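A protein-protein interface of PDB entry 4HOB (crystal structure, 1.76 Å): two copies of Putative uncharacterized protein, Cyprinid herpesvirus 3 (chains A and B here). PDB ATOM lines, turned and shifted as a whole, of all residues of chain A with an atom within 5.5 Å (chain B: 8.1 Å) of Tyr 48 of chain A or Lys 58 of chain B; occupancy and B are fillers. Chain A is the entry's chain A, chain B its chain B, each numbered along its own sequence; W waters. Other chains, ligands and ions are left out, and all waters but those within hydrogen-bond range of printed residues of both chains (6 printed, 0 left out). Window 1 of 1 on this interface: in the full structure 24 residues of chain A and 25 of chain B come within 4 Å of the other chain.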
ATOM      1  N   VAL A  43      -1.715  20.576 -19.209  1.00  0.00           N
ATOM      2  CA  VAL A  43      -2.118  21.974 -19.257  1.00  0.00           C
ATOM      3  C   VAL A  43      -1.656  22.728 -18.013  1.00  0.00           C
ATOM      4  O   VAL A  43      -1.119  23.823 -18.117  1.00  0.00           O
ATOM      5  CB  VAL A  43      -3.644  22.119 -19.437  1.00  0.00           C
ATOM      6  CG1 VAL A  43      -4.086  23.543 -19.149  1.00  0.00           C
ATOM      7  CG2 VAL A  43      -4.050  21.698 -20.847  1.00  0.00           C
ATOM      8  N   ASN A  44      -1.850  22.133 -16.841  1.00  0.00           N
ATOM      9  CA  ASN A  44      -1.398  22.754 -15.598  1.00  0.00           C
ATOM     10  C   ASN A  44       0.119  22.884 -15.531  1.00  0.00           C
ATOM     11  O   ASN A  44       0.639  23.898 -15.065  1.00  0.00           O
ATOM     12  CB  ASN A  44      -1.914  21.986 -14.380  1.00  0.00           C
ATOM     13  CG  ASN A  44      -3.216  22.547 -13.849  1.00  0.00           C
ATOM     14  OD1 ASN A  44      -3.507  23.734 -14.009  1.00  0.00           O
ATOM     15  ND2 ASN A  44      -4.004  21.699 -13.200  1.00  0.00           N
ATOM     16  N   ARG A  45       0.819  21.853 -15.997  1.00  0.00           N
ATOM     17  CA  ARG A  45       2.276  21.869 -16.069  1.00  0.00           C
ATOM     18  C   ARG A  45       2.735  23.093 -16.855  1.00  0.00           C
ATOM     19  O   ARG A  45       3.569  23.889 -16.385  1.00  0.00           O
ATOM     20  CB  ARG A  45       2.781  20.586 -16.738  1.00  0.00           C
ATOM     21  CG  ARG A  45       4.286  20.389 -16.687  1.00  0.00           C
ATOM     22  CD  ARG A  45       4.692  18.995 -17.166  1.00  0.00           C
ATOM     23  NE  ARG A  45       4.500  18.809 -18.603  1.00  0.00           N
ATOM     24  CZ  ARG A  45       3.667  17.923 -19.142  1.00  0.00           C
ATOM     25  NH1 ARG A  45       2.941  17.130 -18.365  1.00  0.00           N
ATOM     26  NH2 ARG A  45       3.565  17.826 -20.460  1.00  0.00           N
ATOM     27  N   HIS A  46       2.160  23.256 -18.044  1.00  0.00           N
ATOM     28  CA  HIS A  46       2.507  24.384 -18.901  1.00  0.00           C
ATOM     29  C   HIS A  46       2.084  25.731 -18.309  1.00  0.00           C
ATOM     30  O   HIS A  46       2.793  26.727 -18.451  1.00  0.00           O
ATOM     31  CB  HIS A  46       1.916  24.200 -20.302  1.00  0.00           C
ATOM     32  CG  HIS A  46       2.571  23.112 -21.094  1.00  0.00           C
ATOM     33  ND1 HIS A  46       2.362  21.774 -20.837  1.00  0.00           N
ATOM     34  CD2 HIS A  46       3.437  23.165 -22.133  1.00  0.00           C
ATOM     35  CE1 HIS A  46       3.068  21.049 -21.686  1.00  0.00           C
ATOM     36  NE2 HIS A  46       3.730  21.869 -22.482  1.00  0.00           N
ATOM     37  N   LEU A  47       0.933  25.754 -17.644  1.00  0.00           N
ATOM     38  CA  LEU A  47       0.411  26.975 -17.037  1.00  0.00           C
ATOM     39  C   LEU A  47       1.308  27.477 -15.918  1.00  0.00           C
ATOM     40  O   LEU A  47       1.566  28.670 -15.816  1.00  0.00           O
ATOM     41  CB  LEU A  47      -1.005  26.759 -16.501  1.00  0.00           C
ATOM     42  CG  LEU A  47      -2.133  26.766 -17.534  1.00  0.00           C
ATOM     43  CD1 LEU A  47      -3.429  26.286 -16.901  1.00  0.00           C
ATOM     44  CD2 LEU A  47      -2.302  28.156 -18.137  1.00  0.00           C
ATOM     45  N   TYR A  48       1.771  26.568 -15.068  1.00  0.00           N
ATOM     46  CA  TYR A  48       2.643  26.965 -13.970  1.00  0.00           C
ATOM     47  C   TYR A  48       4.042  27.308 -14.467  1.00  0.00           C
ATOM     48  O   TYR A  48       4.680  28.238 -13.956  1.00  0.00           O
ATOM     49  CB  TYR A  48       2.658  25.901 -12.871  1.00  0.00           C
ATOM     50  CG  TYR A  48       1.401  25.935 -12.029  1.00  0.00           C
ATOM     51  CD1 TYR A  48       1.221  26.913 -11.059  1.00  0.00           C
ATOM     52  CD2 TYR A  48       0.386  25.003 -12.214  1.00  0.00           C
ATOM     53  CE1 TYR A  48       0.071  26.961 -10.292  1.00  0.00           C
ATOM     54  CE2 TYR A  48      -0.771  25.041 -11.448  1.00  0.00           C
ATOM     55  CZ  TYR A  48      -0.921  26.023 -10.488  1.00  0.00           C
ATOM     56  OH  TYR A  48      -2.067  26.069  -9.723  1.00  0.00           O
ATOM     57  N   ARG A  49       4.504  26.580 -15.484  1.00  0.00           N
ATOM     58  CA  ARG A  49       5.788  26.907 -16.095  1.00  0.00           C
ATOM     59  C   ARG A  49       5.761  28.317 -16.687  1.00  0.00           C
ATOM     60  O   ARG A  49       6.705  29.088 -16.516  1.00  0.00           O
ATOM     61  CB  ARG A  49       6.172  25.880 -17.164  1.00  0.00           C
ATOM     62  CG  ARG A  49       7.602  26.011 -17.661  1.00  0.00           C
ATOM     63  CD  ARG A  49       8.592  25.896 -16.511  1.00  0.00           C
ATOM     64  NE  ARG A  49       8.379  24.680 -15.730  1.00  0.00           N
ATOM     65  CZ  ARG A  49       9.057  23.550 -15.904  1.00  0.00           C
ATOM     66  NH1 ARG A  49      10.003  23.475 -16.830  1.00  0.00           N
ATOM     67  NH2 ARG A  49       8.792  22.494 -15.145  1.00  0.00           N
ATOM     68  N   MET A  50       4.670  28.652 -17.374  1.00  0.00           N
ATOM     69  CA  MET A  50       4.498  29.990 -17.941  1.00  0.00           C
ATOM     70  C   MET A  50       4.288  31.036 -16.854  1.00  0.00           C
ATOM     71  O   MET A  50       4.679  32.192 -17.010  1.00  0.00           O
ATOM     72  CB  MET A  50       3.325  30.024 -18.928  1.00  0.00           C
ATOM     73  CG  MET A  50       3.652  29.467 -20.309  1.00  0.00           C
ATOM     74  SD  MET A  50       2.423  29.919 -21.555  1.00  0.00           S
ATOM     75  CE  MET A  50       1.047  28.868 -21.102  1.00  0.00           C
ATOM     76  N   SER A  51       3.659  30.620 -15.760  1.00  0.00           N
ATOM     77  CA  SER A  51       3.428  31.492 -14.617  1.00  0.00           C
ATOM     78  C   SER A  51       4.756  31.954 -14.044  1.00  0.00           C
ATOM     79  O   SER A  51       4.926  33.132 -13.726  1.00  0.00           O
ATOM     80  CB  SER A  51       2.617  30.768 -13.543  1.00  0.00           C
ATOM     81  OG  SER A  51       2.548  31.533 -12.352  1.00  0.00           O
ATOM     82  N   GLU A  52       5.694  31.018 -13.917  1.00  0.00           N
ATOM     83  CA  GLU A  52       7.045  31.351 -13.473  1.00  0.00           C
ATOM     84  C   GLU A  52       7.668  32.421 -14.365  1.00  0.00           C
ATOM     85  O   GLU A  52       8.348  33.327 -13.881  1.00  0.00           O
ATOM     86  CB  GLU A  52       7.936  30.109 -13.482  1.00  0.00           C
ATOM     87  CG  GLU A  52       7.459  28.984 -12.589  1.00  0.00           C
ATOM     88  CD  GLU A  52       8.280  27.724 -12.771  1.00  0.00           C
ATOM     89  OE1 GLU A  52       7.806  26.640 -12.370  1.00  0.00           O
ATOM     90  OE2 GLU A  52       9.397  27.819 -13.321  1.00  0.00           O
ATOM     91  N   ASP A  53       7.425  32.311 -15.667  1.00  0.00           N
ATOM     92  CA  ASP A  53       8.005  33.229 -16.644  1.00  0.00           C
ATOM     93  C   ASP A  53       7.134  34.460 -16.889  1.00  0.00           C
ATOM     94  O   ASP A  53       7.467  35.313 -17.713  1.00  0.00           O
ATOM     95  CB  ASP A  53       8.282  32.499 -17.961  1.00  0.00           C
ATOM     96  CG  ASP A  53       9.328  31.408 -17.814  1.00  0.00           C
ATOM     97  OD1 ASP A  53      10.304  31.618 -17.063  1.00  0.00           O
ATOM     98  OD2 ASP A  53       9.172  30.341 -18.446  1.00  0.00           O
ATOM     99  N   LYS A  58      -2.858  34.313 -12.664  1.00  0.00           N
ATOM    100  CA  LYS A  58      -4.031  33.633 -12.133  1.00  0.00           C
ATOM    101  C   LYS A  58      -4.693  34.416 -11.003  1.00  0.00           C
ATOM    102  O   LYS A  58      -4.033  35.161 -10.281  1.00  0.00           O
ATOM    103  CB  LYS A  58      -3.668  32.223 -11.658  1.00  0.00           C
ATOM    104  CG  LYS A  58      -2.683  32.178 -10.498  1.00  0.00           C
ATOM    105  CD  LYS A  58      -2.341  30.740 -10.124  1.00  0.00           C
ATOM    106  CE  LYS A  58      -1.531  30.666  -8.837  1.00  0.00           C
ATOM    107  NZ  LYS A  58      -0.220  31.369  -8.936  1.00  0.00           N
ATOM    108  N   PRO A  63      -2.827  31.153  -3.482  1.00  0.00           N
ATOM    109  CA  PRO A  63      -3.847  30.347  -2.807  1.00  0.00           C
ATOM    110  C   PRO A  63      -3.391  29.934  -1.416  1.00  0.00           C
ATOM    111  O   PRO A  63      -2.196  29.979  -1.120  1.00  0.00           O
ATOM    112  CB  PRO A  63      -3.960  29.117  -3.708  1.00  0.00           C
ATOM    113  CG  PRO A  63      -2.604  28.976  -4.301  1.00  0.00           C
ATOM    114  CD  PRO A  63      -2.097  30.382  -4.503  1.00  0.00           C
ATOM    115  N   VAL A  64      -4.338  29.545  -0.571  1.00  0.00           N
ATOM    116  CA  VAL A  64      -4.012  29.051   0.761  1.00  0.00           C
ATOM    117  C   VAL A  64      -4.046  27.530   0.767  1.00  0.00           C
ATOM    118  O   VAL A  64      -5.080  26.927   0.483  1.00  0.00           O
ATOM    119  CB  VAL A  64      -4.989  29.586   1.822  1.00  0.00           C
ATOM    120  CG1 VAL A  64      -4.750  28.894   3.161  1.00  0.00           C
ATOM    121  CG2 VAL A  64      -4.842  31.094   1.963  1.00  0.00           C
ATOM    122  N   TRP A  65      -2.907  26.921   1.079  1.00  0.00           N
ATOM    123  CA  TRP A  65      -2.790  25.468   1.114  1.00  0.00           C
ATOM    124  C   TRP A  65      -3.143  24.921   2.491  1.00  0.00           C
ATOM    125  O   TRP A  65      -2.874  25.559   3.506  1.00  0.00           O
ATOM    126  CB  TRP A  65      -1.368  25.045   0.747  1.00  0.00           C
ATOM    127  CG  TRP A  65      -0.947  25.491  -0.615  1.00  0.00           C
ATOM    128  CD1 TRP A  65      -0.339  26.669  -0.940  1.00  0.00           C
ATOM    129  CD2 TRP A  65      -1.100  24.766  -1.840  1.00  0.00           C
ATOM    130  NE1 TRP A  65      -0.105  26.722  -2.293  1.00  0.00           N
ATOM    131  CE2 TRP A  65      -0.564  25.566  -2.868  1.00  0.00           C
ATOM    132  CE3 TRP A  65      -1.639  23.518  -2.168  1.00  0.00           C
ATOM    133  CZ2 TRP A  65      -0.549  25.159  -4.201  1.00  0.00           C
ATOM    134  CZ3 TRP A  65      -1.622  23.114  -3.496  1.00  0.00           C
ATOM    135  CH2 TRP A  65      -1.084  23.934  -4.495  1.00  0.00           C
ATOM    136  N   TYR A  66      -3.737  23.732   2.524  1.00  0.00           N
ATOM    137  CA  TYR A  66      -4.106  23.106   3.789  1.00  0.00           C
ATOM    138  C   TYR A  66      -4.199  21.590   3.660  1.00  0.00           C
ATOM    139  O   TYR A  66      -4.105  21.045   2.562  1.00  0.00           O
ATOM    140  CB  TYR A  66      -5.424  23.684   4.309  1.00  0.00           C
ATOM    141  CG  TYR A  66      -6.634  23.325   3.475  1.00  0.00           C
ATOM    142  CD1 TYR A  66      -7.537  22.360   3.905  1.00  0.00           C
ATOM    143  CD2 TYR A  66      -6.878  23.954   2.259  1.00  0.00           C
ATOM    144  CE1 TYR A  66      -8.647  22.030   3.150  1.00  0.00           C
ATOM    145  CE2 TYR A  66      -7.983  23.628   1.494  1.00  0.00           C
ATOM    146  CZ  TYR A  66      -8.866  22.669   1.947  1.00  0.00           C
ATOM    147  OH  TYR A  66      -9.967  22.341   1.190  1.00  0.00           O
ATOM    148  N   ALA B  27      -1.838  27.857   4.906  1.00  0.00           N
ATOM    149  CA  ALA B  27      -0.734  28.782   4.709  1.00  0.00           C
ATOM    150  C   ALA B  27      -0.467  29.009   3.235  1.00  0.00           C
ATOM    151  O   ALA B  27      -0.623  28.103   2.417  1.00  0.00           O
ATOM    152  CB  ALA B  27       0.519  28.264   5.391  1.00  0.00           C
ATOM    153  N   ASN B  44       6.404  25.270  -3.970  1.00  0.00           N
ATOM    154  CA  ASN B  44       5.275  25.242  -4.894  1.00  0.00           C
ATOM    155  C   ASN B  44       5.278  23.988  -5.759  1.00  0.00           C
ATOM    156  O   ASN B  44       4.242  23.334  -5.943  1.00  0.00           O
ATOM    157  CB  ASN B  44       5.282  26.484  -5.784  1.00  0.00           C
ATOM    158  CG  ASN B  44       4.624  27.670  -5.124  1.00  0.00           C
ATOM    159  OD1 ASN B  44       3.636  27.521  -4.409  1.00  0.00           O
ATOM    160  ND2 ASN B  44       5.168  28.860  -5.361  1.00  0.00           N
ATOM    161  N   ARG B  45       6.455  23.662  -6.283  1.00  0.00           N
ATOM    162  CA  ARG B  45       6.630  22.480  -7.115  1.00  0.00           C
ATOM    163  C   ARG B  45       6.191  21.220  -6.371  1.00  0.00           C
ATOM    164  O   ARG B  45       5.530  20.352  -6.941  1.00  0.00           O
ATOM    165  CB  ARG B  45       8.085  22.365  -7.570  1.00  0.00           C
ATOM    166  CG  ARG B  45       8.371  21.170  -8.451  1.00  0.00           C
ATOM    167  CD  ARG B  45       9.743  21.281  -9.091  1.00  0.00           C
ATOM    168  NE  ARG B  45      10.283  19.965  -9.412  1.00  0.00           N
ATOM    169  CZ  ARG B  45      11.076  19.271  -8.604  1.00  0.00           C
ATOM    170  NH1 ARG B  45      11.430  19.773  -7.428  1.00  0.00           N
ATOM    171  NH2 ARG B  45      11.515  18.078  -8.970  1.00  0.00           N
ATOM    172  N   LEU B  47       4.113  21.208  -3.697  1.00  0.00           N
ATOM    173  CA  LEU B  47       2.703  21.388  -3.370  1.00  0.00           C
ATOM    174  C   LEU B  47       1.798  20.922  -4.504  1.00  0.00           C
ATOM    175  O   LEU B  47       0.801  20.252  -4.258  1.00  0.00           O
ATOM    176  CB  LEU B  47       2.405  22.852  -3.024  1.00  0.00           C
ATOM    177  CG  LEU B  47       2.836  23.344  -1.638  1.00  0.00           C
ATOM    178  CD1 LEU B  47       2.697  24.859  -1.536  1.00  0.00           C
ATOM    179  CD2 LEU B  47       2.024  22.659  -0.546  1.00  0.00           C
ATOM    180  N   TYR B  48       2.144  21.276  -5.740  1.00  0.00           N
ATOM    181  CA  TYR B  48       1.343  20.875  -6.902  1.00  0.00           C
ATOM    182  C   TYR B  48       1.247  19.348  -7.027  1.00  0.00           C
ATOM    183  O   TYR B  48       0.150  18.772  -7.158  1.00  0.00           O
ATOM    184  CB  TYR B  48       1.935  21.466  -8.186  1.00  0.00           C
ATOM    185  CG  TYR B  48       2.118  22.971  -8.165  1.00  0.00           C
ATOM    186  CD1 TYR B  48       1.280  23.787  -7.413  1.00  0.00           C
ATOM    187  CD2 TYR B  48       3.132  23.575  -8.901  1.00  0.00           C
ATOM    188  CE1 TYR B  48       1.450  25.162  -7.392  1.00  0.00           C
ATOM    189  CE2 TYR B  48       3.308  24.947  -8.886  1.00  0.00           C
ATOM    190  CZ  TYR B  48       2.464  25.735  -8.131  1.00  0.00           C
ATOM    191  OH  TYR B  48       2.635  27.102  -8.114  1.00  0.00           O
ATOM    192  N   SER B  51      -0.782  17.863  -4.341  1.00  0.00           N
ATOM    193  CA  SER B  51      -2.183  18.150  -4.604  1.00  0.00           C
ATOM    194  C   SER B  51      -2.739  17.104  -5.554  1.00  0.00           C
ATOM    195  O   SER B  51      -3.877  16.659  -5.400  1.00  0.00           O
ATOM    196  CB  SER B  51      -2.344  19.547  -5.204  1.00  0.00           C
ATOM    197  OG  SER B  51      -3.712  19.852  -5.411  1.00  0.00           O
ATOM    198  N   GLU B  52      -1.929  16.700  -6.530  1.00  0.00           N
ATOM    199  CA  GLU B  52      -2.360  15.643  -7.448  1.00  0.00           C
ATOM    200  C   GLU B  52      -2.676  14.318  -6.742  1.00  0.00           C
ATOM    201  O   GLU B  52      -3.583  13.593  -7.151  1.00  0.00           O
ATOM    202  CB  GLU B  52      -1.343  15.437  -8.571  1.00  0.00           C
ATOM    203  CG  GLU B  52      -1.331  16.571  -9.579  1.00  0.00           C
ATOM    204  CD  GLU B  52      -2.730  17.041  -9.931  1.00  0.00           C
ATOM    205  OE1 GLU B  52      -3.430  16.328 -10.683  1.00  0.00           O
ATOM    206  OE2 GLU B  52      -3.133  18.121  -9.445  1.00  0.00           O
ATOM    207  N   VAL B  56      -2.490  17.301  -0.203  1.00  0.00           N
ATOM    208  CA  VAL B  56      -2.830  18.648   0.240  1.00  0.00           C
ATOM    209  C   VAL B  56      -4.026  19.164  -0.549  1.00  0.00           C
ATOM    210  O   VAL B  56      -4.383  18.614  -1.592  1.00  0.00           O
ATOM    211  CB  VAL B  56      -1.668  19.650   0.054  1.00  0.00           C
ATOM    212  CG1 VAL B  56      -0.495  19.288   0.948  1.00  0.00           C
ATOM    213  CG2 VAL B  56      -1.245  19.723  -1.409  1.00  0.00           C
ATOM    214  N   ARG B  57      -4.645  20.219  -0.040  1.00  0.00           N
ATOM    215  CA  ARG B  57      -5.715  20.899  -0.756  1.00  0.00           C
ATOM    216  C   ARG B  57      -5.422  22.389  -0.734  1.00  0.00           C
ATOM    217  O   ARG B  57      -4.486  22.827  -0.066  1.00  0.00           O
ATOM    218  CB  ARG B  57      -7.071  20.611  -0.108  1.00  0.00           C
ATOM    219  CG  ARG B  57      -7.503  19.155  -0.176  1.00  0.00           C
ATOM    220  CD  ARG B  57      -8.844  18.952   0.508  1.00  0.00           C
ATOM    221  NE  ARG B  57      -9.331  17.581   0.370  1.00  0.00           N
ATOM    222  CZ  ARG B  57     -10.557  17.262  -0.031  1.00  0.00           C
ATOM    223  NH1 ARG B  57     -11.427  18.215  -0.334  1.00  0.00           N
ATOM    224  NH2 ARG B  57     -10.915  15.988  -0.127  1.00  0.00           N
ATOM    225  N   LYS B  58      -6.215  23.172  -1.456  1.00  0.00           N
ATOM    226  CA  LYS B  58      -5.991  24.610  -1.492  1.00  0.00           C
ATOM    227  C   LYS B  58      -7.277  25.386  -1.737  1.00  0.00           C
ATOM    228  O   LYS B  58      -8.202  24.885  -2.376  1.00  0.00           O
ATOM    229  CB  LYS B  58      -4.949  24.970  -2.552  1.00  0.00           C
ATOM    230  CG  LYS B  58      -5.437  24.809  -3.979  1.00  0.00           C
ATOM    231  CD  LYS B  58      -4.339  25.112  -4.981  1.00  0.00           C
ATOM    232  CE  LYS B  58      -4.890  25.135  -6.393  1.00  0.00           C
ATOM    233  NZ  LYS B  58      -3.815  25.034  -7.411  1.00  0.00           N
ATOM    234  N   HIS B  59      -7.328  26.603  -1.206  1.00  0.00           N
ATOM    235  CA  HIS B  59      -8.439  27.513  -1.445  1.00  0.00           C
ATOM    236  C   HIS B  59      -7.954  28.691  -2.285  1.00  0.00           C
ATOM    237  O   HIS B  59      -6.950  29.318  -1.948  1.00  0.00           O
ATOM    238  CB  HIS B  59      -9.007  28.039  -0.125  1.00  0.00           C
ATOM    239  CG  HIS B  59      -9.680  26.996   0.713  1.00  0.00           C
ATOM    240  ND1 HIS B  59     -10.798  26.306   0.292  1.00  0.00           N
ATOM    241  CD2 HIS B  59      -9.411  26.547   1.962  1.00  0.00           C
ATOM    242  CE1 HIS B  59     -11.181  25.470   1.240  1.00  0.00           C
ATOM    243  NE2 HIS B  59     -10.354  25.595   2.264  1.00  0.00           N
ATOM    244  N   PRO B  60      -8.652  28.980  -3.394  1.00  0.00           N
ATOM    245  CA  PRO B  60      -9.759  28.175  -3.913  1.00  0.00           C
ATOM    246  C   PRO B  60      -9.226  26.943  -4.632  1.00  0.00           C
ATOM    247  O   PRO B  60      -8.023  26.844  -4.873  1.00  0.00           O
ATOM    248  CB  PRO B  60     -10.428  29.114  -4.918  1.00  0.00           C
ATOM    249  CG  PRO B  60      -9.321  29.959  -5.404  1.00  0.00           C
ATOM    250  CD  PRO B  60      -8.427  30.185  -4.210  1.00  0.00           C
ATOM    251  N   GLN B  61     -10.117  26.021  -4.964  1.00  0.00           N
ATOM    252  CA  GLN B  61      -9.726  24.753  -5.565  1.00  0.00           C
ATOM    253  C   GLN B  61      -9.098  24.960  -6.942  1.00  0.00           C
ATOM    254  O   GLN B  61      -8.070  24.361  -7.261  1.00  0.00           O
ATOM    255  CB  GLN B  61     -10.954  23.847  -5.675  1.00  0.00           C
ATOM    256  CG  GLN B  61     -10.671  22.365  -5.602  1.00  0.00           C
ATOM    257  CD  GLN B  61     -11.941  21.558  -5.424  1.00  0.00           C
ATOM    258  OE1 GLN B  61     -12.922  22.043  -4.861  1.00  0.00           O
ATOM    259  NE2 GLN B  61     -11.934  20.323  -5.915  1.00  0.00           N
ATOM    260  N   HIS B  62      -9.720  25.813  -7.751  1.00  0.00           N
ATOM    261  CA  HIS B  62      -9.270  26.043  -9.121  1.00  0.00           C
ATOM    262  C   HIS B  62      -9.171  27.531  -9.424  1.00  0.00           C
ATOM    263  O   HIS B  62     -10.181  28.234  -9.440  1.00  0.00           O
ATOM    264  CB  HIS B  62     -10.233  25.392 -10.112  1.00  0.00           C
ATOM    265  CG  HIS B  62     -10.620  23.995  -9.744  1.00  0.00           C
ATOM    266  ND1 HIS B  62      -9.708  22.964  -9.678  1.00  0.00           N
ATOM    267  CD2 HIS B  62     -11.820  23.459  -9.417  1.00  0.00           C
ATOM    268  CE1 HIS B  62     -10.329  21.853  -9.325  1.00  0.00           C
ATOM    269  NE2 HIS B  62     -11.611  22.125  -9.162  1.00  0.00           N
ATOM    270  N   PRO B  63      -7.948  28.018  -9.669  1.00  0.00           N
ATOM    271  CA  PRO B  63      -7.783  29.439  -9.979  1.00  0.00           C
ATOM    272  C   PRO B  63      -8.232  29.740 -11.403  1.00  0.00           C
ATOM    273  O   PRO B  63      -8.312  28.830 -12.227  1.00  0.00           O
ATOM    274  CB  PRO B  63      -6.274  29.647  -9.843  1.00  0.00           C
ATOM    275  CG  PRO B  63      -5.693  28.321 -10.190  1.00  0.00           C
ATOM    276  CD  PRO B  63      -6.661  27.301  -9.655  1.00  0.00           C
ATOM    277  N   TRP B  65      -7.185  31.441 -14.797  1.00  0.00           N
ATOM    278  CA  TRP B  65      -5.976  31.864 -15.489  1.00  0.00           C
ATOM    279  C   TRP B  65      -6.310  32.912 -16.542  1.00  0.00           C
ATOM    280  O   TRP B  65      -7.366  32.855 -17.159  1.00  0.00           O
ATOM    281  CB  TRP B  65      -5.299  30.667 -16.158  1.00  0.00           C
ATOM    282  CG  TRP B  65      -4.795  29.633 -15.197  1.00  0.00           C
ATOM    283  CD1 TRP B  65      -5.468  28.535 -14.744  1.00  0.00           C
ATOM    284  CD2 TRP B  65      -3.505  29.598 -14.575  1.00  0.00           C
ATOM    285  NE1 TRP B  65      -4.676  27.819 -13.876  1.00  0.00           N
ATOM    286  CE2 TRP B  65      -3.466  28.451 -13.757  1.00  0.00           C
ATOM    287  CE3 TRP B  65      -2.380  30.427 -14.629  1.00  0.00           C
ATOM    288  CZ2 TRP B  65      -2.347  28.113 -13.000  1.00  0.00           C
ATOM    289  CZ3 TRP B  65      -1.267  30.086 -13.880  1.00  0.00           C
ATOM    290  CH2 TRP B  65      -1.261  28.942 -13.072  1.00  0.00           C
HETATM  291  O   HOH W   1     -10.316  22.926  -1.207  1.00  0.00           O
HETATM  292  O   HOH W   2      -2.349  19.411 -12.105  1.00  0.00           O
HETATM  293  O   HOH W   3      -2.876  27.561  -7.846  1.00  0.00           O
HETATM  294  O   HOH W   4      -5.061  25.249 -12.437  1.00  0.00           O
HETATM  295  O   HOH W   5       1.157  28.591  -4.219  1.00  0.00           O
HETATM  296  O   HOH W   6       0.407  28.972  -6.693  1.00  0.00           O
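Among the printed residues, merely in contact across the chains: Leu 47 of chain A with Trp 65 of chain B, Tyr 48 of chain A with Tyr 48 of chain B, Tyr 48 of chain A with Trp 65 of chain B, Ser 51 of chain A with Trp 65 of chain B, Lys 58 of chain A with Trp 65 of chain B, Pro 63 of chain A with His 59 of chain B, Val 64 of chain A with Ala 27 of chain B, Val 64 of chain A with Lys 58 of chain B, Trp 65 of chain A with Leu 47 of chain B, Trp 65 of chain A with Tyr 48 of chain B, Trp 65 of chain A with Val 56 of chain B, Trp 65 of chain A with Arg 57 of chain B, Trp 65 of chain A with Lys 58 of chain B, Tyr 66 of chain A with Val 56 of chain B and Tyr 66 of chain A with Lys 58 of chain B.
Val 43 of chain A touches none of the printed residues of chain B. Of chain B, only Tyr 48 (3.3 Å), Lys 58 (3.1 Å) and Trp 65 (3.6 Å) come within 4 Å of Tyr 48 of chain A. Glu 52 of chain A touches none of the printed residues of chain B. Printed residues of chain B within 4 Å of Pro 63 of chain A: His 59. Of the printed residues of chain B, Val 64 of chain A touches Ala 27, Lys 58 and His 59. Of the printed residues of chain A, Ala 27 of chain B touches Val 64 and Trp 65. Lys 58 of chain B touches just these residues of chain A: Tyr 48 (3.1 Å), Val 64 (3.2 Å), Trp 65 (3.5 Å) and Tyr 66 (3.5 Å). Printed residues of chain A within 4 Å of His 59 of chain B: Pro 63, Val 64 and Tyr 66. The nearest residue of chain A that does not touch Lys 58 of chain B is Pro 63 of chain A (4.2 Å). The nearest printed residue of chain A that does not touch Trp 65 of chain B is Asn 44 of chain A (4.3 Å).
Leu 47 of chain A touches Trp 65 of chain B, and with the chains exchanged Trp 65 of chain A touches Leu 47 of chain B. Tyr 48 of chain B touches its own counterpart, Tyr 48 of chain A. Ser 51 of chain A touches Trp 65 of chain B, but with the chains exchanged Trp 65 of chain A does not touch Ser 51 of chain B (4.02 Å). Lys 58 of chain A touches Trp 65 of chain B, and with the chains exchanged Trp 65 of chain A touches Lys 58 of chain B. Positions printed for both chains: 44, 45, 47, 48, 51, 52, 58, 63 and 65.
The side-chain amino group (NZ) of Lys 58 of chain B lies within hydrogen-bond range of the side-chain hydroxyl (OH) of Tyr 48 of chain A (3.1 Å). The backbone carbonyl oxygen of Val 64 of chain A is in hydrogen-bond range of the backbone NH of His 59 of chain B, at 2.8 Å. The backbone NH (N) of Ala 27 of chain B lies within hydrogen-bond range of the backbone carbonyl oxygen (O) of Trp 65 of chain A (2.9 Å). The backbone NH of Arg 57 of chain B lies within hydrogen-bond range of the backbone carbonyl oxygen of Tyr 66 of chain A, 2.8 Å away. The side-chain hydroxyl of Tyr 66 of chain A sits close to a ring nitrogen (NE2) of His 59 of chain B, at 3.4 Å.
Of the 16 printed residues of chain A, 8 touch a printed residue of chain B. Hydrophobic or aromatic side chains of chain A within 4 Å of the printed part of chain B: Leu 47, Tyr 48, Pro 63, Val 64, Trp 65 and Tyr 66. Along chain A the printed residues that touch a printed residue of chain B span positions 47 to 66. Of the 16 printed residues of chain B, 8 touch a printed residue of chain A. Printed residues of chain B that touch a printed residue of chain A: Ala 27, Leu 47, Tyr 48, Val 56, Arg 57, Lys 58, His 59 and Trp 65. Hydrophobic or aromatic side chains of chain B within 4 Å of the printed part of chain A: Leu 47, Tyr 48, Val 56, His 59 and Trp 65.
Water W1 bridges OH of Tyr 66 of chain A (2.5 Å) and O of Lys 58 of chain B (3.1 Å). Water W3 bridges OH of Tyr 48 of chain A and NZ of Lys 58 of chain B. Water W4 bridges OD1 of Asn 44 of chain A (2.7 Å) and NE1 of Trp 65 of chain B (3.0 Å). Water W2 bridges ND2 of Asn 44 of chain A (3.0 Å) and OE2 of Glu 52 of chain B (3.1 Å). Water W6 lies within hydrogen-bond range of the side-chain hydroxyl (OH) of Tyr 48 of chain B (3.2 Å) and the side-chain amino group (NZ) of Lys 58 of chain A (3.3 Å).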
